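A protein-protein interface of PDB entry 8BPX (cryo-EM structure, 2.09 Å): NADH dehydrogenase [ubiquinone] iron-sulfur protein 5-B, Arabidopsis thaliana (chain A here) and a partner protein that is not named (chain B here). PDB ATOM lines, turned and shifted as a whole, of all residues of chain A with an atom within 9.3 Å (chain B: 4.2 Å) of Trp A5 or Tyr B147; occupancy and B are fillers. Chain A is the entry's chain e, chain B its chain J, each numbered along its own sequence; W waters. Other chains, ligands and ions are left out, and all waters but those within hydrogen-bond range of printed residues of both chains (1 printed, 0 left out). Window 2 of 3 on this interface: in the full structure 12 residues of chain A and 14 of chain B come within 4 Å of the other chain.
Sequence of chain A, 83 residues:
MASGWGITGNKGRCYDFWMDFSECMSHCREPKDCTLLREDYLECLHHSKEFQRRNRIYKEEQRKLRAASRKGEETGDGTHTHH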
ATOM      1  N   ALA A   2     -13.693  15.241  20.761  1.00  0.00           N
ATOM      2  CA  ALA A   2     -13.895  13.848  21.198  1.00  0.00           C
ATOM      3  C   ALA A   2     -13.224  12.740  20.387  1.00  0.00           C
ATOM      4  O   ALA A   2     -13.128  11.718  20.905  1.00  0.00           O
ATOM      5  CB  ALA A   2     -15.386  13.648  21.329  1.00  0.00           C
ATOM      6  N   SER A   3     -12.960  12.979  19.100  1.00  0.00           N
ATOM      7  CA  SER A   3     -12.451  11.909  18.201  1.00  0.00           C
ATOM      8  C   SER A   3     -11.040  11.471  18.585  1.00  0.00           C
ATOM      9  O   SER A   3     -10.708  10.348  18.296  1.00  0.00           O
ATOM     10  CB  SER A   3     -12.509  12.364  16.710  1.00  0.00           C
ATOM     11  OG  SER A   3     -11.397  13.167  16.365  1.00  0.00           O
ATOM     12  N   GLY A   4     -10.221  12.398  19.068  1.00  0.00           N
ATOM     13  CA  GLY A   4      -8.804  12.100  19.319  1.00  0.00           C
ATOM     14  C   GLY A   4      -7.822  12.374  18.192  1.00  0.00           C
ATOM     15  O   GLY A   4      -6.650  12.402  18.462  1.00  0.00           O
ATOM     16  N   TRP A   5      -8.301  12.587  16.951  1.00  0.00           N
ATOM     17  CA  TRP A   5      -7.400  12.881  15.841  1.00  0.00           C
ATOM     18  C   TRP A   5      -7.064  14.370  15.852  1.00  0.00           C
ATOM     19  O   TRP A   5      -7.938  15.212  15.619  1.00  0.00           O
ATOM     20  CB  TRP A   5      -8.028  12.473  14.511  1.00  0.00           C
ATOM     21  CG  TRP A   5      -8.464  11.029  14.414  1.00  0.00           C
ATOM     22  CD1 TRP A   5      -9.734  10.550  14.534  1.00  0.00           C
ATOM     23  CD2 TRP A   5      -7.632   9.892  14.152  1.00  0.00           C
ATOM     24  NE1 TRP A   5      -9.747   9.189  14.368  1.00  0.00           N
ATOM     25  CE2 TRP A   5      -8.470   8.759  14.133  1.00  0.00           C
ATOM     26  CE3 TRP A   5      -6.263   9.722  13.928  1.00  0.00           C
ATOM     27  CZ2 TRP A   5      -7.984   7.475  13.903  1.00  0.00           C
ATOM     28  CZ3 TRP A   5      -5.781   8.447  13.700  1.00  0.00           C
ATOM     29  CH2 TRP A   5      -6.639   7.339  13.689  1.00  0.00           C
ATOM     30  N   GLY A   6      -5.798  14.699  16.115  1.00  0.00           N
ATOM     31  CA  GLY A   6      -5.378  16.084  16.124  1.00  0.00           C
ATOM     32  C   GLY A   6      -5.065  16.616  14.736  1.00  0.00           C
ATOM     33  O   GLY A   6      -4.757  15.875  13.806  1.00  0.00           O
ATOM     34  N   ILE A   7      -5.119  17.923  14.644  1.00  0.00           N
ATOM     35  CA  ILE A   7      -4.955  18.600  13.305  1.00  0.00           C
ATOM     36  C   ILE A   7      -3.497  18.586  12.842  1.00  0.00           C
ATOM     37  O   ILE A   7      -3.303  18.828  11.700  1.00  0.00           O
ATOM     38  CB  ILE A   7      -5.634  19.983  13.305  1.00  0.00           C
ATOM     39  CG1 ILE A   7      -4.926  20.965  14.247  1.00  0.00           C
ATOM     40  CG2 ILE A   7      -7.122  19.859  13.584  1.00  0.00           C
ATOM     41  CD1 ILE A   7      -5.366  22.391  14.100  1.00  0.00           C
ATOM     42  N   THR A   8      -2.552  18.229  13.711  1.00  0.00           N
ATOM     43  CA  THR A   8      -1.144  18.132  13.342  1.00  0.00           C
ATOM     44  C   THR A   8      -0.608  16.705  13.453  1.00  0.00           C
ATOM     45  O   THR A   8       0.608  16.503  13.435  1.00  0.00           O
ATOM     46  CB  THR A   8      -0.295  19.084  14.188  1.00  0.00           C
ATOM     47  OG1 THR A   8      -0.643  18.948  15.569  1.00  0.00           O
ATOM     48  CG2 THR A   8      -0.515  20.531  13.749  1.00  0.00           C
ATOM     49  N   GLY A   9      -1.488  15.715  13.558  1.00  0.00           N
ATOM     50  CA  GLY A   9      -1.066  14.328  13.545  1.00  0.00           C
ATOM     51  C   GLY A   9      -0.721  13.722  14.886  1.00  0.00           C
ATOM     52  O   GLY A   9      -0.061  12.679  14.921  1.00  0.00           O
ATOM     53  N   ASN A  10      -1.132  14.339  15.990  1.00  0.00           N
ATOM     54  CA  ASN A  10      -0.969  13.774  17.323  1.00  0.00           C
ATOM     55  C   ASN A  10      -2.324  13.747  18.020  1.00  0.00           C
ATOM     56  O   ASN A  10      -3.332  14.194  17.473  1.00  0.00           O
ATOM     57  CB  ASN A  10       0.057  14.565  18.143  1.00  0.00           C
ATOM     58  CG  ASN A  10       1.478  14.294  17.704  1.00  0.00           C
ATOM     59  OD1 ASN A  10       1.994  13.192  17.878  1.00  0.00           O
ATOM     60  ND2 ASN A  10       2.116  15.297  17.125  1.00  0.00           N
ATOM     61  N   LYS A  11      -2.342  13.206  19.238  1.00  0.00           N
ATOM     62  CA  LYS A  11      -3.570  13.178  20.021  1.00  0.00           C
ATOM     63  C   LYS A  11      -4.123  14.589  20.186  1.00  0.00           C
ATOM     64  O   LYS A  11      -3.379  15.537  20.441  1.00  0.00           O
ATOM     65  CB  LYS A  11      -3.317  12.547  21.396  1.00  0.00           C
ATOM     66  CG  LYS A  11      -4.497  12.653  22.354  1.00  0.00           C
ATOM     67  CD  LYS A  11      -4.085  12.415  23.805  1.00  0.00           C
ATOM     68  CE  LYS A  11      -3.470  11.040  23.990  1.00  0.00           C
ATOM     69  NZ  LYS A  11      -4.227   9.996  23.255  1.00  0.00           N
ATOM     70  N   GLY A  12      -5.411  14.699  19.921  1.00  0.00           N
ATOM     71  CA  GLY A  12      -6.109  15.980  20.108  1.00  0.00           C
ATOM     72  C   GLY A  12      -5.886  16.606  21.487  1.00  0.00           C
ATOM     73  O   GLY A  12      -5.804  15.824  22.418  1.00  0.00           O
ATOM     74  N   ARG A  13      -5.958  17.931  21.618  1.00  0.00           N
ATOM     75  CA  ARG A  13      -5.657  18.655  22.851  1.00  0.00           C
ATOM     76  C   ARG A  13      -6.573  18.235  23.996  1.00  0.00           C
ATOM     77  O   ARG A  13      -6.119  18.072  25.134  1.00  0.00           O
ATOM     78  CB  ARG A  13      -5.759  20.164  22.611  1.00  0.00           C
ATOM     79  CG  ARG A  13      -6.017  20.979  23.878  1.00  0.00           C
ATOM     80  CD  ARG A  13      -6.043  22.479  23.619  1.00  0.00           C
ATOM     81  NE  ARG A  13      -7.397  23.005  23.510  1.00  0.00           N
ATOM     82  CZ  ARG A  13      -7.938  23.426  22.375  1.00  0.00           C
ATOM     83  NH1 ARG A  13      -7.261  23.405  21.239  1.00  0.00           N
ATOM     84  NH2 ARG A  13      -9.187  23.884  22.380  1.00  0.00           N
ATOM     85  N   CYS A  14      -7.877  18.108  23.721  1.00  0.00           N
ATOM     86  CA  CYS A  14      -8.947  17.842  24.706  1.00  0.00           C
ATOM     87  C   CYS A  14      -9.408  16.365  24.799  1.00  0.00           C
ATOM     88  O   CYS A  14     -10.303  16.113  25.506  1.00  0.00           O
ATOM     89  CB  CYS A  14     -10.121  18.744  24.357  1.00  0.00           C
ATOM     90  SG  CYS A  14      -9.670  20.492  24.319  1.00  0.00           S
ATOM     91  N   TYR A  15      -8.733  15.461  24.154  1.00  0.00           N
ATOM     92  CA  TYR A  15      -9.089  14.028  24.108  1.00  0.00           C
ATOM     93  C   TYR A  15      -8.917  13.293  25.461  1.00  0.00           C
ATOM     94  O   TYR A  15      -9.792  12.560  25.754  1.00  0.00           O
ATOM     95  CB  TYR A  15      -8.309  13.344  22.991  1.00  0.00           C
ATOM     96  CG  TYR A  15      -8.655  11.892  22.878  1.00  0.00           C
ATOM     97  CD1 TYR A  15      -9.895  11.508  22.399  1.00  0.00           C
ATOM     98  CD2 TYR A  15      -7.774  10.920  23.308  1.00  0.00           C
ATOM     99  CE1 TYR A  15     -10.230  10.175  22.283  1.00  0.00           C
ATOM    100  CE2 TYR A  15      -8.087   9.581  23.197  1.00  0.00           C
ATOM    101  CZ  TYR A  15      -9.316   9.218  22.678  1.00  0.00           C
ATOM    102  OH  TYR A  15      -9.649   7.916  22.597  1.00  0.00           O
ATOM    103  N   ASN B 142      -4.476  10.555   6.013  1.00  0.00           N
ATOM    104  CA  ASN B 142      -4.396   9.481   6.991  1.00  0.00           C
ATOM    105  C   ASN B 142      -5.771   8.952   7.392  1.00  0.00           C
ATOM    106  O   ASN B 142      -5.868   7.830   7.899  1.00  0.00           O
ATOM    107  CB  ASN B 142      -3.644   9.986   8.225  1.00  0.00           C
ATOM    108  CG  ASN B 142      -3.416   8.908   9.259  1.00  0.00           C
ATOM    109  OD1 ASN B 142      -2.913   7.830   8.949  1.00  0.00           O
ATOM    110  ND2 ASN B 142      -3.789   9.192  10.499  1.00  0.00           N
ATOM    111  N   LEU B 143      -6.830   9.732   7.182  1.00  0.00           N
ATOM    112  CA  LEU B 143      -8.159   9.395   7.672  1.00  0.00           C
ATOM    113  C   LEU B 143      -9.176   9.089   6.588  1.00  0.00           C
ATOM    114  O   LEU B 143     -10.051   8.251   6.810  1.00  0.00           O
ATOM    115  CB  LEU B 143      -8.717  10.536   8.527  1.00  0.00           C
ATOM    116  CG  LEU B 143      -7.900  10.925   9.752  1.00  0.00           C
ATOM    117  CD1 LEU B 143      -8.547  12.116  10.423  1.00  0.00           C
ATOM    118  CD2 LEU B 143      -7.793   9.746  10.698  1.00  0.00           C
ATOM    119  N   THR B 146      -9.207   5.113   5.192  1.00  0.00           N
ATOM    120  CA  THR B 146      -9.191   3.944   6.062  1.00  0.00           C
ATOM    121  C   THR B 146     -10.252   3.999   7.154  1.00  0.00           C
ATOM    122  O   THR B 146     -11.178   3.185   7.140  1.00  0.00           O
ATOM    123  CB  THR B 146      -7.790   3.793   6.667  1.00  0.00           C
ATOM    124  OG1 THR B 146      -7.384   5.041   7.239  1.00  0.00           O
ATOM    125  CG2 THR B 146      -6.795   3.393   5.593  1.00  0.00           C
ATOM    126  N   TYR B 147     -10.192   4.979   8.056  1.00  0.00           N
ATOM    127  CA  TYR B 147     -11.093   4.991   9.202  1.00  0.00           C
ATOM    128  C   TYR B 147     -12.469   5.538   8.862  1.00  0.00           C
ATOM    129  O   TYR B 147     -13.437   5.208   9.552  1.00  0.00           O
ATOM    130  CB  TYR B 147     -10.466   5.780  10.357  1.00  0.00           C
ATOM    131  CG  TYR B 147      -9.190   5.139  10.845  1.00  0.00           C
ATOM    132  CD1 TYR B 147      -9.228   4.076  11.739  1.00  0.00           C
ATOM    133  CD2 TYR B 147      -7.952   5.558  10.375  1.00  0.00           C
ATOM    134  CE1 TYR B 147      -8.075   3.470  12.169  1.00  0.00           C
ATOM    135  CE2 TYR B 147      -6.791   4.957  10.801  1.00  0.00           C
ATOM    136  CZ  TYR B 147      -6.859   3.912  11.700  1.00  0.00           C
ATOM    137  OH  TYR B 147      -5.712   3.298  12.132  1.00  0.00           O
ATOM    138  N   TYR B 148     -12.585   6.338   7.810  1.00  0.00           N
ATOM    139  CA  TYR B 148     -13.861   6.917   7.415  1.00  0.00           C
ATOM    140  C   TYR B 148     -14.136   6.660   5.939  1.00  0.00           C
ATOM    141  O   TYR B 148     -14.717   7.492   5.240  1.00  0.00           O
ATOM    142  CB  TYR B 148     -13.889   8.407   7.750  1.00  0.00           C
ATOM    143  CG  TYR B 148     -13.740   8.645   9.233  1.00  0.00           C
ATOM    144  CD1 TYR B 148     -14.837   8.557  10.077  1.00  0.00           C
ATOM    145  CD2 TYR B 148     -12.500   8.920   9.797  1.00  0.00           C
ATOM    146  CE1 TYR B 148     -14.712   8.750  11.435  1.00  0.00           C
ATOM    147  CE2 TYR B 148     -12.366   9.120  11.161  1.00  0.00           C
ATOM    148  CZ  TYR B 148     -13.478   9.032  11.973  1.00  0.00           C
ATOM    149  OH  TYR B 148     -13.365   9.229  13.328  1.00  0.00           O
ATOM    150  N   PHE B 149     -13.753   5.473   5.457  1.00  0.00           N
ATOM    151  CA  PHE B 149     -13.824   5.183   4.026  1.00  0.00           C
ATOM    152  C   PHE B 149     -15.263   5.065   3.523  1.00  0.00           C
ATOM    153  O   PHE B 149     -15.527   5.335   2.344  1.00  0.00           O
ATOM    154  CB  PHE B 149     -13.018   3.915   3.711  1.00  0.00           C
ATOM    155  CG  PHE B 149     -13.717   2.630   4.067  1.00  0.00           C
ATOM    156  CD1 PHE B 149     -13.706   2.155   5.368  1.00  0.00           C
ATOM    157  CD2 PHE B 149     -14.364   1.885   3.095  1.00  0.00           C
ATOM    158  CE1 PHE B 149     -14.350   0.976   5.701  1.00  0.00           C
ATOM    159  CE2 PHE B 149     -15.006   0.703   3.419  1.00  0.00           C
ATOM    160  CZ  PHE B 149     -14.998   0.249   4.727  1.00  0.00           C
HETATM  161  O   HOH W   1     -12.062   7.546  14.956  1.00  0.00           O
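Water W1 bridges the side-chain hydroxyl (OH) of Tyr B148 (2.7 Å) and the indole nitrogen (NE1) of Trp A5 (2.9 Å).
Among the printed residues, merely in contact across the chains: Trp A5 with Leu B143 (3.5 Å), Trp A5 with Tyr B147 (3.7 Å), Trp A5 with Tyr B148 (3.8 Å) and Trp A5 with Asn B142 (3.8 Å).
Of the printed residues of chain B, Trp A5 touches Asn B142 (3.8 Å), Leu B143 (3.5 Å), Tyr B147 (3.7 Å) and Tyr B148 (3.8 Å).
Of the printed residues of chain A, Tyr B147 touches Trp A5.
Of chain A, only Trp A5 (3.8 Å) comes within 4 Å of Tyr B148.
Of the printed residues of chain A, Leu B143 touches Trp A5.
Printed residues of chain A within 4 Å of Asn B142: Trp A5 (3.8 Å).
The nearest printed residue of chain A that does not touch Asn B142 is Gly A9 (6.6 Å).
The backbone carbonyl oxygen (O) of Asn B142 lies within hydrogen-bond range of the side-chain hydroxyl (OG1) of Thr B146.
The backbone NH (N) of Tyr B148 lies within hydrogen-bond range of the backbone carbonyl oxygen (O) of Leu B143 (3.3 Å).
The side-chain hydroxyl (OG) of Ser A3 is in hydrogen-bond range of the backbone NH (N) of Trp A5 (3.2 Å).
Hydrophobic or aromatic side chains of chain A that line the printed part of chain B: Trp A5.
Among the printed residues, no Asp or Glu carboxylate lies within 4 Å of a Lys or Arg side-chain nitrogen of the other chain.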
